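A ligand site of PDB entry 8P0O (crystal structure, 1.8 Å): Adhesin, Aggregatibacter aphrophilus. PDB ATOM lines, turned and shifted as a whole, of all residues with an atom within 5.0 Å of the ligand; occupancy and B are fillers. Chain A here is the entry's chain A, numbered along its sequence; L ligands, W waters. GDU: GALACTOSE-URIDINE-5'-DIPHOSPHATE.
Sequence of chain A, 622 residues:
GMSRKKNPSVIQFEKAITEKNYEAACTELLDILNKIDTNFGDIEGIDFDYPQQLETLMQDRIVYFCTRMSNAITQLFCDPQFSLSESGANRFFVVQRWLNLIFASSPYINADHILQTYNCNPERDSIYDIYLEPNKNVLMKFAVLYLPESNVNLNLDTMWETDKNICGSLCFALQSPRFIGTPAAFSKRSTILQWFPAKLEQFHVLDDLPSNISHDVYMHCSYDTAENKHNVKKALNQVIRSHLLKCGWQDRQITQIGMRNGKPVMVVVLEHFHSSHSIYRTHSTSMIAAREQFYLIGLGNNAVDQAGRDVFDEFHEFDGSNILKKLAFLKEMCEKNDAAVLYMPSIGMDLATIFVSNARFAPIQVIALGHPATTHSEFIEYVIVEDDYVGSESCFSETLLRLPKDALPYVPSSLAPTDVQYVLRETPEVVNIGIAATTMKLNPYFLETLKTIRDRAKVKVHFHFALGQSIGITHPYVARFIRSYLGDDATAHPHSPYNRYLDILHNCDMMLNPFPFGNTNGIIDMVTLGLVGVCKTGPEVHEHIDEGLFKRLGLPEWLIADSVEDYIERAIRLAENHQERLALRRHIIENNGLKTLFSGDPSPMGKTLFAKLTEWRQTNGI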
ATOM      1  N   HIS A 277     -34.794 -17.179 -11.090  1.00  0.00           N
ATOM      2  CA  HIS A 277     -34.213 -17.795 -12.272  1.00  0.00           C
ATOM      3  C   HIS A 277     -33.202 -16.866 -12.949  1.00  0.00           C
ATOM      4  O   HIS A 277     -33.359 -15.642 -12.890  1.00  0.00           O
ATOM      5  CB  HIS A 277     -35.337 -18.195 -13.234  1.00  0.00           C
ATOM      6  CG  HIS A 277     -34.887 -19.086 -14.353  1.00  0.00           C
ATOM      7  ND1 HIS A 277     -34.182 -18.608 -15.448  1.00  0.00           N
ATOM      8  CD2 HIS A 277     -35.029 -20.415 -14.550  1.00  0.00           C
ATOM      9  CE1 HIS A 277     -33.895 -19.609 -16.275  1.00  0.00           C
ATOM     10  NE2 HIS A 277     -34.421 -20.726 -15.743  1.00  0.00           N
ATOM     11  N   SER A 278     -32.223 -17.454 -13.669  1.00  0.00           N
ATOM     12  CA  SER A 278     -31.213 -16.690 -14.408  1.00  0.00           C
ATOM     13  C   SER A 278     -31.862 -15.686 -15.343  1.00  0.00           C
ATOM     14  O   SER A 278     -31.336 -14.590 -15.528  1.00  0.00           O
ATOM     15  CB  SER A 278     -30.272 -17.552 -15.247  1.00  0.00           C
ATOM     16  OG  SER A 278     -29.712 -18.553 -14.463  1.00  0.00           O
ATOM     17  N   MET A 349     -37.408 -23.837 -23.768  1.00  0.00           N
ATOM     18  CA  MET A 349     -37.678 -24.549 -22.546  1.00  0.00           C
ATOM     19  C   MET A 349     -39.120 -25.052 -22.506  1.00  0.00           C
ATOM     20  O   MET A 349     -39.403 -25.987 -21.763  1.00  0.00           O
ATOM     21  CB  MET A 349     -37.332 -23.684 -21.327  1.00  0.00           C
ATOM     22  CG  MET A 349     -35.843 -23.335 -21.329  1.00  0.00           C
ATOM     23  SD  MET A 349     -35.325 -22.080 -20.161  1.00  0.00           S
ATOM     24  CE  MET A 349     -33.660 -21.668 -20.726  1.00  0.00           C
ATOM     25  N   GLY A 370     -31.892 -16.420 -23.657  1.00  0.00           N
ATOM     26  CA  GLY A 370     -32.066 -17.260 -22.477  1.00  0.00           C
ATOM     27  C   GLY A 370     -31.659 -18.717 -22.740  1.00  0.00           C
ATOM     28  O   GLY A 370     -31.007 -19.318 -21.893  1.00  0.00           O
ATOM     29  N   HIS A 371     -32.000 -19.258 -23.904  1.00  0.00           N
ATOM     30  CA  HIS A 371     -31.306 -20.400 -24.480  1.00  0.00           C
ATOM     31  C   HIS A 371     -30.507 -19.869 -25.677  1.00  0.00           C
ATOM     32  O   HIS A 371     -31.073 -19.453 -26.672  1.00  0.00           O
ATOM     33  CB  HIS A 371     -32.258 -21.519 -24.894  1.00  0.00           C
ATOM     34  CG  HIS A 371     -31.516 -22.735 -25.370  1.00  0.00           C
ATOM     35  ND1 HIS A 371     -30.670 -23.470 -24.561  1.00  0.00           N
ATOM     36  CD2 HIS A 371     -31.479 -23.318 -26.588  1.00  0.00           C
ATOM     37  CE1 HIS A 371     -30.141 -24.463 -25.284  1.00  0.00           C
ATOM     38  NE2 HIS A 371     -30.618 -24.391 -26.509  1.00  0.00           N
ATOM     39  N   PRO A 372     -29.163 -19.836 -25.609  1.00  0.00           N
ATOM     40  CA  PRO A 372     -28.359 -19.125 -26.614  1.00  0.00           C
ATOM     41  C   PRO A 372     -28.126 -19.850 -27.939  1.00  0.00           C
ATOM     42  O   PRO A 372     -27.053 -20.405 -28.177  1.00  0.00           O
ATOM     43  CB  PRO A 372     -27.034 -18.898 -25.882  1.00  0.00           C
ATOM     44  CG  PRO A 372     -26.944 -20.025 -24.878  1.00  0.00           C
ATOM     45  CD  PRO A 372     -28.368 -20.270 -24.445  1.00  0.00           C
ATOM     46  N   THR A 438     -23.291 -28.096 -16.115  1.00  0.00           N
ATOM     47  CA  THR A 438     -24.398 -29.009 -16.308  1.00  0.00           C
ATOM     48  C   THR A 438     -23.891 -30.171 -17.154  1.00  0.00           C
ATOM     49  O   THR A 438     -22.967 -30.033 -17.970  1.00  0.00           O
ATOM     50  CB  THR A 438     -25.639 -28.387 -16.982  1.00  0.00           C
ATOM     51  OG1 THR A 438     -25.263 -27.631 -18.131  1.00  0.00           O
ATOM     52  CG2 THR A 438     -26.470 -27.490 -16.091  1.00  0.00           C
ATOM     53  N   LYS A 441     -23.240 -30.039 -20.994  1.00  0.00           N
ATOM     54  CA  LYS A 441     -22.015 -29.399 -21.486  1.00  0.00           C
ATOM     55  C   LYS A 441     -20.822 -30.346 -21.572  1.00  0.00           C
ATOM     56  O   LYS A 441     -19.781 -29.964 -22.110  1.00  0.00           O
ATOM     57  CB  LYS A 441     -21.643 -28.187 -20.630  1.00  0.00           C
ATOM     58  CG  LYS A 441     -22.720 -27.127 -20.593  1.00  0.00           C
ATOM     59  CD  LYS A 441     -22.427 -25.927 -19.726  1.00  0.00           C
ATOM     60  CE  LYS A 441     -23.566 -24.948 -19.634  1.00  0.00           C
ATOM     61  NZ  LYS A 441     -23.170 -23.742 -18.868  1.00  0.00           N
ATOM     62  N   ALA A 466     -18.489 -30.287 -10.531  1.00  0.00           N
ATOM     63  CA  ALA A 466     -19.731 -29.905  -9.865  1.00  0.00           C
ATOM     64  C   ALA A 466     -20.856 -29.987 -10.883  1.00  0.00           C
ATOM     65  O   ALA A 466     -21.011 -29.099 -11.717  1.00  0.00           O
ATOM     66  CB  ALA A 466     -19.576 -28.519  -9.252  1.00  0.00           C
ATOM     67  N   LEU A 467     -21.587 -31.128 -10.869  1.00  0.00           N
ATOM     68  CA  LEU A 467     -22.383 -31.524 -12.041  1.00  0.00           C
ATOM     69  C   LEU A 467     -23.871 -31.194 -11.880  1.00  0.00           C
ATOM     70  O   LEU A 467     -24.652 -32.006 -11.323  1.00  0.00           O
ATOM     71  CB  LEU A 467     -22.196 -33.037 -12.221  1.00  0.00           C
ATOM     72  CG  LEU A 467     -20.791 -33.494 -12.583  1.00  0.00           C
ATOM     73  CD1 LEU A 467     -20.525 -34.898 -12.157  1.00  0.00           C
ATOM     74  CD2 LEU A 467     -20.564 -33.359 -14.064  1.00  0.00           C
ATOM     75  N   GLY A 468     -24.289 -30.049 -12.391  1.00  0.00           N
ATOM     76  CA  GLY A 468     -25.698 -29.700 -12.516  1.00  0.00           C
ATOM     77  C   GLY A 468     -26.432 -30.765 -13.322  1.00  0.00           C
ATOM     78  O   GLY A 468     -25.941 -31.188 -14.360  1.00  0.00           O
ATOM     79  N   PRO A 494     -22.342 -35.074  -7.415  1.00  0.00           N
ATOM     80  CA  PRO A 494     -23.727 -34.891  -7.811  1.00  0.00           C
ATOM     81  C   PRO A 494     -24.224 -33.459  -7.602  1.00  0.00           C
ATOM     82  O   PRO A 494     -23.656 -32.707  -6.822  1.00  0.00           O
ATOM     83  CB  PRO A 494     -24.540 -35.824  -6.902  1.00  0.00           C
ATOM     84  CG  PRO A 494     -23.518 -36.791  -6.367  1.00  0.00           C
ATOM     85  CD  PRO A 494     -22.202 -36.060  -6.327  1.00  0.00           C
ATOM     86  N   HIS A 495     -25.281 -33.106  -8.326  1.00  0.00           N
ATOM     87  CA  HIS A 495     -25.984 -31.855  -8.187  1.00  0.00           C
ATOM     88  C   HIS A 495     -26.229 -31.626  -6.695  1.00  0.00           C
ATOM     89  O   HIS A 495     -26.713 -32.519  -6.000  1.00  0.00           O
ATOM     90  CB  HIS A 495     -27.321 -31.914  -8.913  1.00  0.00           C
ATOM     91  CG  HIS A 495     -27.968 -30.597  -9.139  1.00  0.00           C
ATOM     92  ND1 HIS A 495     -28.312 -29.713  -8.130  1.00  0.00           N
ATOM     93  CD2 HIS A 495     -28.379 -30.055 -10.279  1.00  0.00           C
ATOM     94  CE1 HIS A 495     -28.854 -28.622  -8.665  1.00  0.00           C
ATOM     95  NE2 HIS A 495     -28.924 -28.815  -9.979  1.00  0.00           N
ATOM     96  N   SER A 496     -25.908 -30.434  -6.213  1.00  0.00           N
ATOM     97  CA  SER A 496     -25.903 -30.206  -4.778  1.00  0.00           C
ATOM     98  C   SER A 496     -26.572 -28.853  -4.488  1.00  0.00           C
ATOM     99  O   SER A 496     -26.733 -28.036  -5.388  1.00  0.00           O
ATOM    100  CB  SER A 496     -24.506 -30.247  -4.251  1.00  0.00           C
ATOM    101  OG  SER A 496     -23.790 -29.104  -4.738  1.00  0.00           O
ATOM    102  N   PRO A 497     -26.995 -28.602  -3.242  1.00  0.00           N
ATOM    103  CA  PRO A 497     -27.476 -27.274  -2.854  1.00  0.00           C
ATOM    104  C   PRO A 497     -26.367 -26.255  -3.090  1.00  0.00           C
ATOM    105  O   PRO A 497     -25.182 -26.586  -3.037  1.00  0.00           O
ATOM    106  CB  PRO A 497     -27.743 -27.386  -1.331  1.00  0.00           C
ATOM    107  CG  PRO A 497     -27.862 -28.877  -1.064  1.00  0.00           C
ATOM    108  CD  PRO A 497     -27.009 -29.570  -2.123  1.00  0.00           C
ATOM    109  N   TYR A 498     -26.755 -25.006  -3.287  1.00  0.00           N
ATOM    110  CA  TYR A 498     -25.838 -23.940  -3.673  1.00  0.00           C
ATOM    111  C   TYR A 498     -24.642 -23.815  -2.724  1.00  0.00           C
ATOM    112  O   TYR A 498     -23.505 -23.720  -3.198  1.00  0.00           O
ATOM    113  CB  TYR A 498     -26.600 -22.628  -3.829  1.00  0.00           C
ATOM    114  CG  TYR A 498     -25.753 -21.498  -4.363  1.00  0.00           C
ATOM    115  CD1 TYR A 498     -25.153 -21.605  -5.612  1.00  0.00           C
ATOM    116  CD2 TYR A 498     -25.538 -20.327  -3.647  1.00  0.00           C
ATOM    117  CE1 TYR A 498     -24.336 -20.599  -6.112  1.00  0.00           C
ATOM    118  CE2 TYR A 498     -24.742 -19.309  -4.151  1.00  0.00           C
ATOM    119  CZ  TYR A 498     -24.141 -19.445  -5.383  1.00  0.00           C
ATOM    120  OH  TYR A 498     -23.370 -18.451  -5.935  1.00  0.00           O
ATOM    121  N   TYR A 501     -22.163 -26.640  -3.248  1.00  0.00           N
ATOM    122  CA  TYR A 501     -21.573 -26.384  -4.552  1.00  0.00           C
ATOM    123  C   TYR A 501     -20.468 -25.342  -4.448  1.00  0.00           C
ATOM    124  O   TYR A 501     -19.380 -25.568  -4.946  1.00  0.00           O
ATOM    125  CB  TYR A 501     -22.684 -25.985  -5.506  1.00  0.00           C
ATOM    126  CG  TYR A 501     -22.296 -25.233  -6.753  1.00  0.00           C
ATOM    127  CD1 TYR A 501     -21.928 -25.884  -7.921  1.00  0.00           C
ATOM    128  CD2 TYR A 501     -22.300 -23.853  -6.774  1.00  0.00           C
ATOM    129  CE1 TYR A 501     -21.580 -25.180  -9.069  1.00  0.00           C
ATOM    130  CE2 TYR A 501     -21.936 -23.131  -7.902  1.00  0.00           C
ATOM    131  CZ  TYR A 501     -21.577 -23.794  -9.062  1.00  0.00           C
ATOM    132  OH  TYR A 501     -21.230 -23.047 -10.168  1.00  0.00           O
ATOM    133  N   PHE A 517     -20.137 -25.470 -25.480  1.00  0.00           N
ATOM    134  CA  PHE A 517     -21.098 -24.641 -24.816  1.00  0.00           C
ATOM    135  C   PHE A 517     -20.515 -24.258 -23.454  1.00  0.00           C
ATOM    136  O   PHE A 517     -20.381 -25.090 -22.557  1.00  0.00           O
ATOM    137  CB  PHE A 517     -22.422 -25.399 -24.798  1.00  0.00           C
ATOM    138  CG  PHE A 517     -23.652 -24.588 -24.515  1.00  0.00           C
ATOM    139  CD1 PHE A 517     -23.797 -23.896 -23.308  1.00  0.00           C
ATOM    140  CD2 PHE A 517     -24.737 -24.649 -25.379  1.00  0.00           C
ATOM    141  CE1 PHE A 517     -24.957 -23.201 -23.037  1.00  0.00           C
ATOM    142  CE2 PHE A 517     -25.895 -23.953 -25.084  1.00  0.00           C
ATOM    143  CZ  PHE A 517     -25.995 -23.228 -23.936  1.00  0.00           C
ATOM    144  N   ASN A 521     -23.371 -18.279 -15.517  1.00  0.00           N
ATOM    145  CA  ASN A 521     -23.466 -18.311 -14.075  1.00  0.00           C
ATOM    146  C   ASN A 521     -22.183 -18.863 -13.455  1.00  0.00           C
ATOM    147  O   ASN A 521     -21.742 -18.416 -12.394  1.00  0.00           O
ATOM    148  CB  ASN A 521     -24.631 -19.166 -13.611  1.00  0.00           C
ATOM    149  CG  ASN A 521     -25.968 -18.479 -13.831  1.00  0.00           C
ATOM    150  OD1 ASN A 521     -26.170 -17.353 -13.383  1.00  0.00           O
ATOM    151  ND2 ASN A 521     -26.881 -19.189 -14.464  1.00  0.00           N
ATOM    152  N   GLY A 522     -21.588 -19.876 -14.063  1.00  0.00           N
ATOM    153  CA  GLY A 522     -20.416 -20.499 -13.493  1.00  0.00           C
ATOM    154  C   GLY A 522     -19.223 -19.539 -13.430  1.00  0.00           C
ATOM    155  O   GLY A 522     -18.374 -19.675 -12.556  1.00  0.00           O
ATOM    156  N   ASP A 525     -19.866 -17.366 -10.427  1.00  0.00           N
ATOM    157  CA  ASP A 525     -19.508 -18.143  -9.254  1.00  0.00           C
ATOM    158  C   ASP A 525     -17.995 -18.137  -9.100  1.00  0.00           C
ATOM    159  O   ASP A 525     -17.493 -18.006  -7.993  1.00  0.00           O
ATOM    160  CB  ASP A 525     -20.033 -19.602  -9.365  1.00  0.00           C
ATOM    161  CG  ASP A 525     -21.552 -19.721  -9.389  1.00  0.00           C
ATOM    162  OD1 ASP A 525     -22.201 -18.841  -8.845  1.00  0.00           O
ATOM    163  OD2 ASP A 525     -22.067 -20.679 -10.013  1.00  0.00           O
HETATM  164  N1  GDU L   1     -25.873 -24.972  -9.026  1.00  0.00           N
HETATM  165  C2  GDU L   1     -26.003 -25.453  -7.736  1.00  0.00           C
HETATM  166  N3  GDU L   1     -25.524 -26.720  -7.526  1.00  0.00           N
HETATM  167  C4  GDU L   1     -24.976 -27.574  -8.470  1.00  0.00           C
HETATM  168  C5  GDU L   1     -24.829 -26.981  -9.777  1.00  0.00           C
HETATM  169  C6  GDU L   1     -25.298 -25.744 -10.012  1.00  0.00           C
HETATM  170  O2  GDU L   1     -26.476 -24.766  -6.841  1.00  0.00           O
HETATM  171  O4  GDU L   1     -24.550 -28.671  -8.127  1.00  0.00           O
HETATM  172  C1D GDU L   1     -26.402 -23.593  -9.282  1.00  0.00           C
HETATM  173  C2D GDU L   1     -25.393 -22.465  -9.095  1.00  0.00           C
HETATM  174  O2D GDU L   1     -26.085 -21.316  -8.638  1.00  0.00           O
HETATM  175  C3D GDU L   1     -24.863 -22.247 -10.515  1.00  0.00           C
HETATM  176  C4D GDU L   1     -26.141 -22.485 -11.323  1.00  0.00           C
HETATM  177  O4D GDU L   1     -26.856 -23.533 -10.610  1.00  0.00           O
HETATM  178  O3D GDU L   1     -24.425 -20.909 -10.740  1.00  0.00           O
HETATM  179  C5D GDU L   1     -25.958 -22.918 -12.755  1.00  0.00           C
HETATM  180  O5D GDU L   1     -27.287 -22.848 -13.350  1.00  0.00           O
HETATM  181  PA  GDU L   1     -27.848 -24.150 -14.076  1.00  0.00           P
HETATM  182  O1A GDU L   1     -27.596 -25.347 -13.198  1.00  0.00           O
HETATM  183  O2A GDU L   1     -29.257 -23.926 -14.540  1.00  0.00           O
HETATM  184  O3A GDU L   1     -26.742 -24.102 -15.289  1.00  0.00           O
HETATM  185  PB  GDU L   1     -26.375 -22.932 -16.308  1.00  0.00           P
HETATM  186  O1B GDU L   1     -25.641 -23.486 -17.508  1.00  0.00           O
HETATM  187  O2B GDU L   1     -25.670 -21.783 -15.626  1.00  0.00           O
HETATM  188  O3B GDU L   1     -27.871 -22.531 -16.768  1.00  0.00           O
HETATM  189  C1' GDU L   1     -28.307 -21.207 -17.064  1.00  0.00           C
HETATM  190  C2' GDU L   1     -29.807 -21.142 -16.745  1.00  0.00           C
HETATM  191  C3' GDU L   1     -30.619 -21.924 -17.804  1.00  0.00           C
HETATM  192  C4' GDU L   1     -30.299 -21.360 -19.188  1.00  0.00           C
HETATM  193  C5' GDU L   1     -28.796 -21.542 -19.443  1.00  0.00           C
HETATM  194  C6' GDU L   1     -28.324 -21.023 -20.785  1.00  0.00           C
HETATM  195  O2' GDU L   1     -29.985 -21.634 -15.424  1.00  0.00           O
HETATM  196  O3' GDU L   1     -32.022 -21.857 -17.567  1.00  0.00           O
HETATM  197  O4' GDU L   1     -30.640 -19.968 -19.268  1.00  0.00           O
HETATM  198  O5' GDU L   1     -28.052 -20.825 -18.418  1.00  0.00           O
HETATM  199  O6' GDU L   1     -27.079 -21.643 -21.097  1.00  0.00           O
HETATM  200  O   HOH W   1     -30.456 -23.432 -21.947  1.00  0.00           O
HETATM  201  O   HOH W   2     -25.341 -19.618 -17.076  1.00  0.00           O
HETATM  202  O   HOH W   3     -22.619 -24.141 -12.393  1.00  0.00           O
HETATM  203  O   HOH W   4     -22.818 -21.515 -16.163  1.00  0.00           O
HETATM  204  O   HOH W   5     -27.139 -25.499 -18.740  1.00  0.00           O
HETATM  205  O   HOH W   6     -24.742 -21.267 -19.416  1.00  0.00           O
HETATM  206  O   HOH W   7     -22.236 -30.324  -7.604  1.00  0.00           O
HETATM  207  O   HOH W   8     -23.531 -25.137 -16.150  1.00  0.00           O
HETATM  208  O   HOH W   9     -22.833 -27.028 -12.415  1.00  0.00           O
HETATM  209  O   HOH W  10     -24.974 -26.374 -13.552  1.00  0.00           O
HETATM  210  O   HOH W  11     -29.550 -25.502 -17.604  1.00  0.00           O
HETATM  211  O   HOH W  12     -29.033 -26.633  -6.166  1.00  0.00           O
HETATM  212  O   HOH W  13     -27.644 -24.458 -21.111  1.00  0.00           O
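An oxygen (O3D) of the ligand lies within hydrogen-bond range of the side-chain carboxylate of Asp 525. O of Gly 370 sits at hydrogen-bond distance from O4' of the ligand (2.7 Å). An oxygen (O4) of the ligand is in hydrogen-bond range of the backbone NH (N) of Ser 496 (2.9 Å). The backbone carbonyl oxygen (O) of Ser 496 is in hydrogen-bond range of a nitrogen (N3) of the ligand (2.8 Å). OG of Ser 496 is in hydrogen-bond range of O4 of the ligand (3.5 Å). The side-chain amino group (NZ) of Lys 441 is in salt-bridge range of an oxygen (O1B) of the ligand, 2.8 Å away. The side-chain amide nitrogen (ND2) of Asn 521 lies within hydrogen-bond range of an oxygen (O2B) of the ligand (3.1 Å). NE2 of His 277 lies close to O3' of the ligand. An oxygen (O2') of the ligand sits at hydrogen-bond distance from the side-chain hydroxyl (OG) of Ser 278 (3.2 Å).
The side-chain carboxylate of Asp 525 is in hydrogen-bond range of the side-chain hydroxyl of Tyr 498, 3.2 Å away. The side-chain carboxylate (OD2) of Asp 525 sits at hydrogen-bond distance from the side-chain hydroxyl (OH) of Tyr 501, at 2.5 Å. OG of Ser 496 lies within hydrogen-bond range of N of Tyr 501. ND2 of Asn 521 lies within hydrogen-bond range of OG of Ser 278, at 2.9 Å. The backbone NH (N) of His 495 is in hydrogen-bond range of the backbone carbonyl oxygen (O) of Leu 467 (3.3 Å).
Residues that only touch the ligand: Tyr 498, Phe 517, Thr 438, His 495, Tyr 501, Met 349, Pro 372 and Gly 468. Hydrophobic or aromatic side chains that line the ligand: His 277, Met 349, Pro 372, Tyr 498, Tyr 501 and Phe 517. Of the 21 residues printed, 15 come within 4 Å of the ligand. Along chain A the residues within 4 Å of the ligand span positions 277 to 525. The nearest printed residue that does not touch the ligand is Pro 497 (4.04 Å).
Water W2 lies within hydrogen-bond range of O2B of the ligand (2.6 Å) and N of Asn 521 (2.8 Å). Water W5 lies within hydrogen-bond range of an oxygen (O1B) of the ligand (2.8 Å) and the side-chain hydroxyl (OG1) of Thr 438 (2.9 Å). Water W6 bridges O6' of the ligand (2.9 Å) and NZ of Lys 441 (3.0 Å). Water W4 lies within hydrogen-bond range of O2B of the ligand (2.9 Å), N of Gly 522 (2.9 Å) and N of Asn 521 (3.3 Å). Water W8 lies within hydrogen-bond range of the backbone NH of Thr 438, an oxygen (O1B) of the ligand and the side-chain amino group of Lys 441. Water W12 lies within hydrogen-bond range of O of Ser 496 and O2 of the ligand.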
